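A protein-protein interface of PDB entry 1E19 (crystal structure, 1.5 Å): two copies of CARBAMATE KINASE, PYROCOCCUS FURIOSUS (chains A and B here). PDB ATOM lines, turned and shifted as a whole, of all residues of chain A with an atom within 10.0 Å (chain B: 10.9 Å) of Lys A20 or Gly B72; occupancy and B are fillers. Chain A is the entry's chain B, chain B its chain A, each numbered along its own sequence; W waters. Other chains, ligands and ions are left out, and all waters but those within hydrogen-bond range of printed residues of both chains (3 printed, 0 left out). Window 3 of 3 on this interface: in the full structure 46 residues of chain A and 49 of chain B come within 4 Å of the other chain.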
ATOM      1  N   LEU A  14     -12.281 -28.138 -19.078  1.00  0.00           N
ATOM      2  CA  LEU A  14     -13.290 -28.937 -18.359  1.00  0.00           C
ATOM      3  C   LEU A  14     -14.685 -28.938 -18.941  1.00  0.00           C
ATOM      4  O   LEU A  14     -15.409 -29.934 -18.690  1.00  0.00           O
ATOM      5  CB  LEU A  14     -13.386 -28.360 -16.899  1.00  0.00           C
ATOM      6  CG  LEU A  14     -12.059 -28.172 -16.146  1.00  0.00           C
ATOM      7  CD1 LEU A  14     -12.345 -27.636 -14.717  1.00  0.00           C
ATOM      8  CD2 LEU A  14     -11.217 -29.446 -16.109  1.00  0.00           C
ATOM      9  N   GLN A  15     -15.123 -27.859 -19.612  1.00  0.00           N
ATOM     10  CA  GLN A  15     -16.478 -27.730 -20.124  1.00  0.00           C
ATOM     11  C   GLN A  15     -16.484 -27.021 -21.463  1.00  0.00           C
ATOM     12  O   GLN A  15     -15.751 -26.047 -21.606  1.00  0.00           O
ATOM     13  CB  GLN A  15     -17.308 -26.870 -19.133  1.00  0.00           C
ATOM     14  CG  GLN A  15     -17.571 -27.567 -17.839  1.00  0.00           C
ATOM     15  CD  GLN A  15     -18.508 -27.052 -16.760  1.00  0.00           C
ATOM     16  OE1 GLN A  15     -19.477 -26.306 -16.983  1.00  0.00           O
ATOM     17  NE2 GLN A  15     -18.212 -27.509 -15.513  1.00  0.00           N
ATOM     18  N   GLN A  16     -17.379 -27.488 -22.323  1.00  0.00           N
ATOM     19  CA  GLN A  16     -17.485 -26.772 -23.635  1.00  0.00           C
ATOM     20  C   GLN A  16     -18.718 -25.885 -23.517  1.00  0.00           C
ATOM     21  O   GLN A  16     -19.563 -25.945 -22.622  1.00  0.00           O
ATOM     22  CB  GLN A  16     -17.434 -27.662 -24.848  1.00  0.00           C
ATOM     23  CG  GLN A  16     -16.147 -28.439 -25.042  1.00  0.00           C
ATOM     24  CD  GLN A  16     -14.901 -27.611 -24.702  1.00  0.00           C
ATOM     25  OE1 GLN A  16     -13.941 -28.172 -24.156  1.00  0.00           O
ATOM     26  NE2 GLN A  16     -14.854 -26.334 -25.073  1.00  0.00           N
ATOM     27  N   ARG A  17     -18.785 -24.977 -24.510  1.00  0.00           N
ATOM     28  CA  ARG A  17     -19.880 -24.028 -24.598  1.00  0.00           C
ATOM     29  C   ARG A  17     -21.198 -24.776 -24.641  1.00  0.00           C
ATOM     30  O   ARG A  17     -21.325 -25.715 -25.421  1.00  0.00           O
ATOM     31  CB  ARG A  17     -19.757 -23.095 -25.823  1.00  0.00           C
ATOM     32  CG  ARG A  17     -20.739 -21.916 -25.600  1.00  0.00           C
ATOM     33  CD  ARG A  17     -20.964 -21.182 -26.904  1.00  0.00           C
ATOM     34  NE  ARG A  17     -19.697 -20.773 -27.503  1.00  0.00           N
ATOM     35  CZ  ARG A  17     -18.932 -19.752 -27.130  1.00  0.00           C
ATOM     36  NH1 ARG A  17     -19.258 -18.942 -26.135  1.00  0.00           N
ATOM     37  NH2 ARG A  17     -17.806 -19.551 -27.815  1.00  0.00           N
ATOM     38  N   GLY A  18     -22.117 -24.419 -23.758  1.00  0.00           N
ATOM     39  CA  GLY A  18     -23.414 -25.058 -23.696  1.00  0.00           C
ATOM     40  C   GLY A  18     -23.517 -26.274 -22.797  1.00  0.00           C
ATOM     41  O   GLY A  18     -24.614 -26.802 -22.610  1.00  0.00           O
ATOM     42  N   GLN A  19     -22.409 -26.806 -22.271  1.00  0.00           N
ATOM     43  CA  GLN A  19     -22.469 -28.001 -21.441  1.00  0.00           C
ATOM     44  C   GLN A  19     -22.774 -27.678 -19.984  1.00  0.00           C
ATOM     45  O   GLN A  19     -22.341 -26.597 -19.526  1.00  0.00           O
ATOM     46  CB  GLN A  19     -21.099 -28.705 -21.499  1.00  0.00           C
ATOM     47  CG  GLN A  19     -20.904 -29.411 -22.857  1.00  0.00           C
ATOM     48  CD  GLN A  19     -19.645 -30.226 -22.877  1.00  0.00           C
ATOM     49  OE1 GLN A  19     -18.698 -29.852 -22.134  1.00  0.00           O
ATOM     50  NE2 GLN A  19     -19.512 -31.288 -23.643  1.00  0.00           N
ATOM     51  N   LYS A  20     -23.545 -28.510 -19.293  1.00  0.00           N
ATOM     52  CA  LYS A  20     -23.823 -28.226 -17.880  1.00  0.00           C
ATOM     53  C   LYS A  20     -22.711 -28.684 -16.948  1.00  0.00           C
ATOM     54  O   LYS A  20     -22.644 -28.319 -15.762  1.00  0.00           O
ATOM     55  CB  LYS A  20     -25.160 -28.848 -17.459  1.00  0.00           C
ATOM     56  CG  LYS A  20     -26.364 -28.021 -17.936  1.00  0.00           C
ATOM     57  CD  LYS A  20     -27.506 -28.263 -16.945  1.00  0.00           C
ATOM     58  CE  LYS A  20     -28.877 -28.021 -17.553  1.00  0.00           C
ATOM     59  NZ  LYS A  20     -29.818 -29.131 -17.176  1.00  0.00           N
ATOM     60  N   GLY A  21     -21.802 -29.522 -17.431  1.00  0.00           N
ATOM     61  CA  GLY A  21     -20.692 -29.961 -16.583  1.00  0.00           C
ATOM     62  C   GLY A  21     -21.054 -31.237 -15.886  1.00  0.00           C
ATOM     63  O   GLY A  21     -20.715 -31.550 -14.731  1.00  0.00           O
ATOM     64  N   SER A  22     -21.836 -32.063 -16.632  1.00  0.00           N
ATOM     65  CA  SER A  22     -22.061 -33.383 -16.057  1.00  0.00           C
ATOM     66  C   SER A  22     -20.709 -34.050 -15.978  1.00  0.00           C
ATOM     67  O   SER A  22     -19.602 -33.849 -16.502  1.00  0.00           O
ATOM     68  CB  SER A  22     -22.980 -34.196 -17.047  1.00  0.00           C
ATOM     69  OG  SER A  22     -22.248 -34.515 -18.234  1.00  0.00           O
ATOM     70  N   TYR A  23     -20.714 -35.141 -15.158  1.00  0.00           N
ATOM     71  CA  TYR A  23     -19.548 -35.936 -14.976  1.00  0.00           C
ATOM     72  C   TYR A  23     -18.924 -36.530 -16.269  1.00  0.00           C
ATOM     73  O   TYR A  23     -17.764 -36.521 -16.558  1.00  0.00           O
ATOM     74  CB  TYR A  23     -19.932 -37.050 -13.997  1.00  0.00           C
ATOM     75  CG  TYR A  23     -18.894 -38.076 -13.878  1.00  0.00           C
ATOM     76  CD1 TYR A  23     -17.660 -37.971 -13.275  1.00  0.00           C
ATOM     77  CD2 TYR A  23     -19.192 -39.327 -14.501  1.00  0.00           C
ATOM     78  CE1 TYR A  23     -16.689 -38.898 -13.113  1.00  0.00           C
ATOM     79  CE2 TYR A  23     -18.250 -40.292 -14.350  1.00  0.00           C
ATOM     80  CZ  TYR A  23     -17.051 -40.119 -13.770  1.00  0.00           C
ATOM     81  OH  TYR A  23     -16.172 -41.145 -13.753  1.00  0.00           O
ATOM     82  N   GLU A  24     -19.879 -37.104 -17.077  1.00  0.00           N
ATOM     83  CA  GLU A  24     -19.381 -37.594 -18.377  1.00  0.00           C
ATOM     84  C   GLU A  24     -18.811 -36.524 -19.305  1.00  0.00           C
ATOM     85  O   GLU A  24     -17.799 -36.825 -19.953  1.00  0.00           O
ATOM     86  CB  GLU A  24     -20.682 -38.125 -19.066  1.00  0.00           C
ATOM     87  CG  GLU A  24     -21.499 -39.163 -18.352  1.00  0.00           C
ATOM     88  CD  GLU A  24     -22.135 -38.881 -17.002  1.00  0.00           C
ATOM     89  OE1 GLU A  24     -22.742 -37.857 -16.618  1.00  0.00           O
ATOM     90  OE2 GLU A  24     -22.044 -39.928 -16.255  1.00  0.00           O
ATOM     91  N   GLU A  25     -19.420 -35.340 -19.303  1.00  0.00           N
ATOM     92  CA  GLU A  25     -18.862 -34.253 -20.116  1.00  0.00           C
ATOM     93  C   GLU A  25     -17.445 -33.891 -19.642  1.00  0.00           C
ATOM     94  O   GLU A  25     -16.510 -33.680 -20.426  1.00  0.00           O
ATOM     95  CB  GLU A  25     -19.722 -32.989 -20.043  1.00  0.00           C
ATOM     96  CG  GLU A  25     -21.035 -33.284 -20.802  1.00  0.00           C
ATOM     97  CD  GLU A  25     -22.071 -32.241 -20.512  1.00  0.00           C
ATOM     98  OE1 GLU A  25     -22.070 -31.505 -19.481  1.00  0.00           O
ATOM     99  OE2 GLU A  25     -23.010 -32.097 -21.324  1.00  0.00           O
ATOM    100  N   MET A  26     -17.363 -33.766 -18.297  1.00  0.00           N
ATOM    101  CA  MET A  26     -16.069 -33.327 -17.784  1.00  0.00           C
ATOM    102  C   MET A  26     -15.009 -34.373 -17.979  1.00  0.00           C
ATOM    103  O   MET A  26     -13.873 -34.060 -18.251  1.00  0.00           O
ATOM    104  CB  MET A  26     -16.241 -33.007 -16.246  1.00  0.00           C
ATOM    105  CG  MET A  26     -17.037 -31.706 -16.083  1.00  0.00           C
ATOM    106  SD  MET A  26     -17.159 -31.247 -14.290  1.00  0.00           S
ATOM    107  CE  MET A  26     -15.476 -30.992 -13.920  1.00  0.00           C
ATOM    108  N   ASN A  29     -13.747 -33.947 -21.592  1.00  0.00           N
ATOM    109  CA  ASN A  29     -12.957 -32.781 -21.820  1.00  0.00           C
ATOM    110  C   ASN A  29     -11.587 -32.873 -21.173  1.00  0.00           C
ATOM    111  O   ASN A  29     -10.526 -32.479 -21.617  1.00  0.00           O
ATOM    112  CB  ASN A  29     -13.675 -31.535 -21.268  1.00  0.00           C
ATOM    113  CG  ASN A  29     -14.931 -31.181 -22.065  1.00  0.00           C
ATOM    114  OD1 ASN A  29     -14.808 -31.252 -23.329  1.00  0.00           O
ATOM    115  ND2 ASN A  29     -16.058 -30.887 -21.490  1.00  0.00           N
ATOM    116  N   GLY A  54     -14.373 -21.456 -11.947  1.00  0.00           N
ATOM    117  CA  GLY A  54     -15.626 -20.667 -11.773  1.00  0.00           C
ATOM    118  C   GLY A  54     -16.924 -21.439 -11.886  1.00  0.00           C
ATOM    119  O   GLY A  54     -17.741 -21.307 -10.933  1.00  0.00           O
ATOM    120  N   PRO A  55     -17.114 -22.217 -12.929  1.00  0.00           N
ATOM    121  CA  PRO A  55     -18.356 -22.958 -13.058  1.00  0.00           C
ATOM    122  C   PRO A  55     -18.463 -24.027 -11.991  1.00  0.00           C
ATOM    123  O   PRO A  55     -19.537 -24.378 -11.560  1.00  0.00           O
ATOM    124  CB  PRO A  55     -18.281 -23.645 -14.443  1.00  0.00           C
ATOM    125  CG  PRO A  55     -17.389 -22.673 -15.155  1.00  0.00           C
ATOM    126  CD  PRO A  55     -16.294 -22.287 -14.166  1.00  0.00           C
ATOM    127  N   GLN A  56     -17.334 -24.587 -11.506  1.00  0.00           N
ATOM    128  CA  GLN A  56     -17.347 -25.659 -10.533  1.00  0.00           C
ATOM    129  C   GLN A  56     -17.660 -25.168  -9.116  1.00  0.00           C
ATOM    130  O   GLN A  56     -18.519 -25.724  -8.450  1.00  0.00           O
ATOM    131  CB  GLN A  56     -15.970 -26.387 -10.620  1.00  0.00           C
ATOM    132  CG  GLN A  56     -15.826 -27.200 -11.935  1.00  0.00           C
ATOM    133  CD  GLN A  56     -15.442 -26.310 -13.120  1.00  0.00           C
ATOM    134  OE1 GLN A  56     -15.882 -26.538 -14.321  1.00  0.00           O
ATOM    135  NE2 GLN A  56     -14.646 -25.307 -12.942  1.00  0.00           N
ATOM    136  N   VAL A  57     -17.070 -24.044  -8.727  1.00  0.00           N
ATOM    137  CA  VAL A  57     -17.456 -23.435  -7.441  1.00  0.00           C
ATOM    138  C   VAL A  57     -18.915 -22.944  -7.612  1.00  0.00           C
ATOM    139  O   VAL A  57     -19.614 -23.145  -6.627  1.00  0.00           O
ATOM    140  CB  VAL A  57     -16.588 -22.186  -7.167  1.00  0.00           C
ATOM    141  CG1 VAL A  57     -17.143 -21.340  -5.999  1.00  0.00           C
ATOM    142  CG2 VAL A  57     -15.163 -22.582  -6.750  1.00  0.00           C
ATOM    143  N   GLY A  58     -19.226 -22.419  -8.835  1.00  0.00           N
ATOM    144  CA  GLY A  58     -20.676 -21.964  -8.901  1.00  0.00           C
ATOM    145  C   GLY A  58     -21.664 -23.172  -8.706  1.00  0.00           C
ATOM    146  O   GLY A  58     -22.630 -22.912  -7.956  1.00  0.00           O
ATOM    147  N   SER A  59     -21.348 -24.288  -9.352  1.00  0.00           N
ATOM    148  CA  SER A  59     -22.259 -25.441  -9.100  1.00  0.00           C
ATOM    149  C   SER A  59     -22.313 -25.851  -7.648  1.00  0.00           C
ATOM    150  O   SER A  59     -23.361 -26.157  -7.084  1.00  0.00           O
ATOM    151  CB  SER A  59     -21.750 -26.600  -9.961  1.00  0.00           C
ATOM    152  OG  SER A  59     -21.863 -26.275 -11.373  1.00  0.00           O
ATOM    153  N   LEU A  60     -21.139 -25.884  -6.946  1.00  0.00           N
ATOM    154  CA  LEU A  60     -21.189 -26.197  -5.516  1.00  0.00           C
ATOM    155  C   LEU A  60     -22.002 -25.187  -4.661  1.00  0.00           C
ATOM    156  O   LEU A  60     -22.649 -25.712  -3.770  1.00  0.00           O
ATOM    157  CB  LEU A  60     -19.724 -26.340  -5.012  1.00  0.00           C
ATOM    158  CG  LEU A  60     -18.989 -27.635  -5.484  1.00  0.00           C
ATOM    159  CD1 LEU A  60     -17.480 -27.424  -5.287  1.00  0.00           C
ATOM    160  CD2 LEU A  60     -19.475 -28.804  -4.635  1.00  0.00           C
ATOM    161  N   LEU A  62     -24.543 -23.497  -5.790  1.00  0.00           N
ATOM    162  CA  LEU A  62     -25.971 -23.821  -6.110  1.00  0.00           C
ATOM    163  C   LEU A  62     -26.467 -25.017  -5.336  1.00  0.00           C
ATOM    164  O   LEU A  62     -27.436 -25.154  -4.590  1.00  0.00           O
ATOM    165  CB  LEU A  62     -26.183 -24.056  -7.608  1.00  0.00           C
ATOM    166  CG  LEU A  62     -26.043 -22.844  -8.551  1.00  0.00           C
ATOM    167  CD1 LEU A  62     -25.845 -23.181 -10.008  1.00  0.00           C
ATOM    168  CD2 LEU A  62     -27.254 -21.940  -8.319  1.00  0.00           C
ATOM    169  N   HIS A  63     -25.633 -26.125  -5.353  1.00  0.00           N
ATOM    170  CA  HIS A  63     -25.957 -27.334  -4.655  1.00  0.00           C
ATOM    171  C   HIS A  63     -26.191 -27.073  -3.186  1.00  0.00           C
ATOM    172  O   HIS A  63     -27.094 -27.672  -2.539  1.00  0.00           O
ATOM    173  CB  HIS A  63     -24.879 -28.423  -4.831  1.00  0.00           C
ATOM    174  CG  HIS A  63     -24.859 -29.100  -6.185  1.00  0.00           C
ATOM    175  ND1 HIS A  63     -23.742 -29.304  -6.942  1.00  0.00           N
ATOM    176  CD2 HIS A  63     -25.934 -29.732  -6.726  1.00  0.00           C
ATOM    177  CE1 HIS A  63     -24.096 -30.064  -8.040  1.00  0.00           C
ATOM    178  NE2 HIS A  63     -25.378 -30.278  -7.814  1.00  0.00           N
ATOM    179  N   ALA A  66     -29.315 -25.298  -2.259  1.00  0.00           N
ATOM    180  CA  ALA A  66     -30.474 -26.209  -2.321  1.00  0.00           C
ATOM    181  C   ALA A  66     -30.476 -27.230  -1.199  1.00  0.00           C
ATOM    182  O   ALA A  66     -31.470 -27.620  -0.592  1.00  0.00           O
ATOM    183  CB  ALA A  66     -30.405 -26.923  -3.688  1.00  0.00           C
ATOM    184  N   TRP A  88     -11.834 -31.977  -6.375  1.00  0.00           N
ATOM    185  CA  TRP A  88     -12.627 -32.509  -7.558  1.00  0.00           C
ATOM    186  C   TRP A  88     -11.815 -32.431  -8.855  1.00  0.00           C
ATOM    187  O   TRP A  88     -11.602 -33.489  -9.511  1.00  0.00           O
ATOM    188  CB  TRP A  88     -13.859 -31.611  -7.614  1.00  0.00           C
ATOM    189  CG  TRP A  88     -14.793 -31.837  -8.781  1.00  0.00           C
ATOM    190  CD1 TRP A  88     -14.748 -32.798  -9.796  1.00  0.00           C
ATOM    191  CD2 TRP A  88     -15.908 -31.026  -9.061  1.00  0.00           C
ATOM    192  NE1 TRP A  88     -15.857 -32.611 -10.614  1.00  0.00           N
ATOM    193  CE2 TRP A  88     -16.593 -31.521 -10.186  1.00  0.00           C
ATOM    194  CE3 TRP A  88     -16.470 -29.877  -8.434  1.00  0.00           C
ATOM    195  CZ2 TRP A  88     -17.736 -30.928 -10.755  1.00  0.00           C
ATOM    196  CZ3 TRP A  88     -17.594 -29.282  -8.971  1.00  0.00           C
ATOM    197  CH2 TRP A  88     -18.213 -29.821 -10.052  1.00  0.00           C
ATOM    198  N   HIS B  63     -26.517 -32.523  -0.585  1.00  0.00           N
ATOM    199  CA  HIS B  63     -26.476 -31.262  -1.313  1.00  0.00           C
ATOM    200  C   HIS B  63     -26.684 -31.472  -2.779  1.00  0.00           C
ATOM    201  O   HIS B  63     -27.418 -30.721  -3.474  1.00  0.00           O
ATOM    202  CB  HIS B  63     -25.141 -30.507  -1.110  1.00  0.00           C
ATOM    203  CG  HIS B  63     -24.929 -29.890   0.230  1.00  0.00           C
ATOM    204  ND1 HIS B  63     -25.811 -28.988   0.843  1.00  0.00           N
ATOM    205  CD2 HIS B  63     -23.867 -30.003   1.072  1.00  0.00           C
ATOM    206  CE1 HIS B  63     -25.255 -28.632   2.009  1.00  0.00           C
ATOM    207  NE2 HIS B  63     -24.114 -29.245   2.204  1.00  0.00           N
ATOM    208  N   MET B  64     -25.948 -32.458  -3.444  1.00  0.00           N
ATOM    209  CA  MET B  64     -26.067 -32.601  -4.895  1.00  0.00           C
ATOM    210  C   MET B  64     -27.416 -33.250  -5.299  1.00  0.00           C
ATOM    211  O   MET B  64     -27.830 -32.864  -6.401  1.00  0.00           O
ATOM    212  CB  MET B  64     -24.880 -33.453  -5.447  1.00  0.00           C
ATOM    213  CG  MET B  64     -23.542 -32.658  -5.269  1.00  0.00           C
ATOM    214  SD  MET B  64     -22.149 -33.531  -6.059  1.00  0.00           S
ATOM    215  CE  MET B  64     -21.867 -34.932  -4.989  1.00  0.00           C
ATOM    216  N   ASP B  65     -27.986 -34.066  -4.424  1.00  0.00           N
ATOM    217  CA  ASP B  65     -29.342 -34.561  -4.891  1.00  0.00           C
ATOM    218  C   ASP B  65     -30.223 -33.315  -4.807  1.00  0.00           C
ATOM    219  O   ASP B  65     -31.098 -33.276  -5.683  1.00  0.00           O
ATOM    220  CB  ASP B  65     -29.850 -35.520  -3.831  1.00  0.00           C
ATOM    221  CG  ASP B  65     -31.163 -36.279  -4.284  1.00  0.00           C
ATOM    222  OD1 ASP B  65     -30.916 -37.130  -5.166  1.00  0.00           O
ATOM    223  OD2 ASP B  65     -32.062 -35.956  -3.581  1.00  0.00           O
ATOM    224  N   ALA B  66     -30.151 -32.434  -3.842  1.00  0.00           N
ATOM    225  CA  ALA B  66     -31.070 -31.269  -3.754  1.00  0.00           C
ATOM    226  C   ALA B  66     -30.742 -30.375  -4.908  1.00  0.00           C
ATOM    227  O   ALA B  66     -31.625 -29.728  -5.593  1.00  0.00           O
ATOM    228  CB  ALA B  66     -30.961 -30.597  -2.395  1.00  0.00           C
ATOM    229  N   GLY B  67     -29.501 -30.030  -5.284  1.00  0.00           N
ATOM    230  CA  GLY B  67     -29.130 -29.188  -6.386  1.00  0.00           C
ATOM    231  C   GLY B  67     -29.692 -29.639  -7.734  1.00  0.00           C
ATOM    232  O   GLY B  67     -30.143 -28.854  -8.617  1.00  0.00           O
ATOM    233  N   GLN B  68     -29.603 -30.946  -7.985  1.00  0.00           N
ATOM    234  CA  GLN B  68     -30.070 -31.502  -9.301  1.00  0.00           C
ATOM    235  C   GLN B  68     -31.600 -31.381  -9.199  1.00  0.00           C
ATOM    236  O   GLN B  68     -32.110 -31.011 -10.266  1.00  0.00           O
ATOM    237  CB  GLN B  68     -29.558 -32.934  -9.407  1.00  0.00           C
ATOM    238  CG  GLN B  68     -29.928 -33.769 -10.635  1.00  0.00           C
ATOM    239  CD  GLN B  68     -29.048 -35.043 -10.631  1.00  0.00           C
ATOM    240  OE1 GLN B  68     -28.108 -35.194 -11.459  1.00  0.00           O
ATOM    241  NE2 GLN B  68     -29.484 -35.880  -9.676  1.00  0.00           N
ATOM    242  N   ALA B  69     -32.235 -31.706  -8.117  1.00  0.00           N
ATOM    243  CA  ALA B  69     -33.705 -31.569  -8.009  1.00  0.00           C
ATOM    244  C   ALA B  69     -34.202 -30.135  -8.116  1.00  0.00           C
ATOM    245  O   ALA B  69     -35.242 -29.851  -8.769  1.00  0.00           O
ATOM    246  CB  ALA B  69     -34.205 -32.169  -6.726  1.00  0.00           C
ATOM    247  N   THR B  70     -33.544 -29.143  -7.556  1.00  0.00           N
ATOM    248  CA  THR B  70     -33.986 -27.731  -7.612  1.00  0.00           C
ATOM    249  C   THR B  70     -33.536 -26.977  -8.800  1.00  0.00           C
ATOM    250  O   THR B  70     -34.380 -26.226  -9.410  1.00  0.00           O
ATOM    251  CB  THR B  70     -33.417 -27.097  -6.314  1.00  0.00           C
ATOM    252  OG1 THR B  70     -33.951 -27.807  -5.199  1.00  0.00           O
ATOM    253  CG2 THR B  70     -33.729 -25.615  -6.202  1.00  0.00           C
ATOM    254  N   TYR B  71     -32.310 -26.968  -9.283  1.00  0.00           N
ATOM    255  CA  TYR B  71     -31.699 -26.192 -10.279  1.00  0.00           C
ATOM    256  C   TYR B  71     -31.345 -26.938 -11.555  1.00  0.00           C
ATOM    257  O   TYR B  71     -30.963 -26.339 -12.586  1.00  0.00           O
ATOM    258  CB  TYR B  71     -30.409 -25.542  -9.766  1.00  0.00           C
ATOM    259  CG  TYR B  71     -30.611 -24.586  -8.626  1.00  0.00           C
ATOM    260  CD1 TYR B  71     -31.390 -23.412  -8.838  1.00  0.00           C
ATOM    261  CD2 TYR B  71     -30.028 -24.739  -7.370  1.00  0.00           C
ATOM    262  CE1 TYR B  71     -31.547 -22.526  -7.784  1.00  0.00           C
ATOM    263  CE2 TYR B  71     -30.191 -23.838  -6.343  1.00  0.00           C
ATOM    264  CZ  TYR B  71     -30.979 -22.714  -6.556  1.00  0.00           C
ATOM    265  OH  TYR B  71     -31.149 -21.825  -5.500  1.00  0.00           O
ATOM    266  N   GLY B  72     -31.537 -28.268 -11.544  1.00  0.00           N
ATOM    267  CA  GLY B  72     -31.289 -29.081 -12.691  1.00  0.00           C
ATOM    268  C   GLY B  72     -29.826 -29.240 -13.050  1.00  0.00           C
ATOM    269  O   GLY B  72     -29.543 -29.629 -14.178  1.00  0.00           O
ATOM    270  N   ILE B  73     -28.978 -28.908 -12.078  1.00  0.00           N
ATOM    271  CA  ILE B  73     -27.530 -29.082 -12.373  1.00  0.00           C
ATOM    272  C   ILE B  73     -27.181 -30.544 -12.012  1.00  0.00           C
ATOM    273  O   ILE B  73     -27.726 -31.122 -11.082  1.00  0.00           O
ATOM    274  CB  ILE B  73     -26.705 -28.033 -11.652  1.00  0.00           C
ATOM    275  CG1 ILE B  73     -26.894 -28.086 -10.153  1.00  0.00           C
ATOM    276  CG2 ILE B  73     -27.047 -26.637 -12.256  1.00  0.00           C
ATOM    277  CD1 ILE B  73     -25.876 -27.226  -9.380  1.00  0.00           C
ATOM    278  N   PRO B  74     -26.126 -31.050 -12.666  1.00  0.00           N
ATOM    279  CA  PRO B  74     -25.773 -32.430 -12.508  1.00  0.00           C
ATOM    280  C   PRO B  74     -25.192 -32.851 -11.146  1.00  0.00           C
ATOM    281  O   PRO B  74     -24.422 -31.984 -10.678  1.00  0.00           O
ATOM    282  CB  PRO B  74     -24.733 -32.748 -13.575  1.00  0.00           C
ATOM    283  CG  PRO B  74     -24.397 -31.466 -14.195  1.00  0.00           C
ATOM    284  CD  PRO B  74     -25.438 -30.424 -13.805  1.00  0.00           C
ATOM    285  N   ALA B  75     -25.629 -33.957 -10.581  1.00  0.00           N
ATOM    286  CA  ALA B  75     -24.909 -34.400  -9.340  1.00  0.00           C
ATOM    287  C   ALA B  75     -23.707 -35.160  -9.861  1.00  0.00           C
ATOM    288  O   ALA B  75     -23.741 -35.824 -10.899  1.00  0.00           O
ATOM    289  CB  ALA B  75     -25.832 -35.318  -8.512  1.00  0.00           C
ATOM    290  N   GLN B  76     -22.684 -35.247  -8.992  1.00  0.00           N
ATOM    291  CA  GLN B  76     -21.427 -35.993  -9.366  1.00  0.00           C
ATOM    292  C   GLN B  76     -21.450 -37.272  -8.548  1.00  0.00           C
ATOM    293  O   GLN B  76     -21.997 -37.441  -7.473  1.00  0.00           O
ATOM    294  CB  GLN B  76     -20.262 -35.146  -8.896  1.00  0.00           C
ATOM    295  CG  GLN B  76     -20.220 -33.734  -9.585  1.00  0.00           C
ATOM    296  CD  GLN B  76     -20.016 -33.892 -11.094  1.00  0.00           C
ATOM    297  OE1 GLN B  76     -19.329 -34.768 -11.526  1.00  0.00           O
ATOM    298  NE2 GLN B  76     -20.498 -32.936 -11.854  1.00  0.00           N
HETATM  299  O   HOH W   1     -34.074 -26.624  -2.538  1.00  0.00           O
HETATM  300  O   HOH W   2     -17.171 -34.102 -12.836  1.00  0.00           O
HETATM  301  O   HOH W   3     -23.064 -35.840 -13.615  1.00  0.00           O
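Of the printed residues of chain B, Lys A20 touches Gly B72 (3.1 Å) and Pro B74 (3.9 Å).
Printed residues of chain A within 4 Å of Gly B72: Lys A20.
No residue of chain B comes within 4 Å of Gln A19.
Printed residues of chain B within 4 Å of Gly A21: Pro B74 (3.7 Å) and Gln B76 (3.2 Å).
Printed residues of chain A within 4 Å of Thr B70: Ala A66 (3.95 Å).
Of the printed residues of chain A, Met B64 touches His A63 (3.4 Å).
Of the printed residues of chain A, Gly B67 touches His A63 (3.3 Å) and Ala A66 (3.6 Å).
Of the printed residues of chain A, Pro B74 touches Lys A20, Gly A21, Ser A22 and His A63.
Gln B68 touches none of the printed residues of chain A.
The nearest residue of chain B that does not touch Lys A20 is Ile B73 (4.6 Å).
The nearest printed residue of chain A that does not touch His B63 is Ala A66 (4.8 Å).
Among the printed residues, pairs that only touch across the chains: Lys A20 with Pro B74, Gly A21 with Pro B74, Ser A22 with Pro B74, Tyr A23 with Gln B76, Ser A59 with Ile B73, Leu A62 with Tyr B71, Leu A62 with Ile B73, His A63 with Met B64, His A63 with Gly B67, His A63 with Ile B73, Ala A66 with Ala B66, Ala A66 with Gly B67, Ala A66 with Thr B70 and Trp A88 with Gln B76.
A ring nitrogen (ND1) of His A63 is in hydrogen-bond range of the backbone carbonyl oxygen of Ser A59 (3.2 Å).
OE1 of Glu A25 lies within hydrogen-bond range of N of Lys A20 (3.3 Å).
The backbone carbonyl oxygen of Pro A55 sits at hydrogen-bond distance from the side-chain hydroxyl of Ser A59 (3.0 Å).
N of Gln B76 sits at hydrogen-bond distance from SD of Met B64, 3.4 Å away.
The backbone carbonyl oxygen (O) of Gly B67 lies within hydrogen-bond range of the backbone NH (N) of Gly B72, 3.3 Å away.
The backbone NH (N) of Ser A22 is in hydrogen-bond range of the side-chain carboxylate (OE1) of Glu A25 (2.9 Å).
His B63 touches its own counterpart, His A63.
Ala B66 touches its own counterpart, Ala A66.
Positions printed for both chains: 63 and 66.
Of the 14 printed residues of chain B, 10 touch a printed residue of chain A.
Hydrophobic or aromatic side chains of chain B that line the printed part of chain A: His B63, Met B64, Ala B66, Tyr B71, Ile B73 and Pro B74.
Along chain B the printed residues that touch a printed residue of chain A span positions 63 to 76.
Among the printed residues, no Asp or Glu carboxylate lies within 4 Å of a Lys or Arg side-chain nitrogen of the other chain.
Water W2 lies within hydrogen-bond range of OE1 of Gln B76, NE1 of Trp A88 and SD of Met A26.
Water W3 lies within hydrogen-bond range of O of Ala B75 and N of Tyr A23.
Water W1 lies within hydrogen-bond range of OG1 of Thr B70 (2.9 Å) and O of Ala A66 (3.4 Å).
O of Gly A21 lies within hydrogen-bond range of NE2 of Gln B76.
The backbone carbonyl oxygen (O) of His A63 lies close to the backbone carbonyl oxygen (O) of His B63, 3.2 Å away.
NE2 of His A63 sits close to O of Pro B74 (3.5 Å).
The backbone carbonyl oxygen (O) of Gly B72 is in hydrogen-bond range of the side-chain amino group (NZ) of Lys A20.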
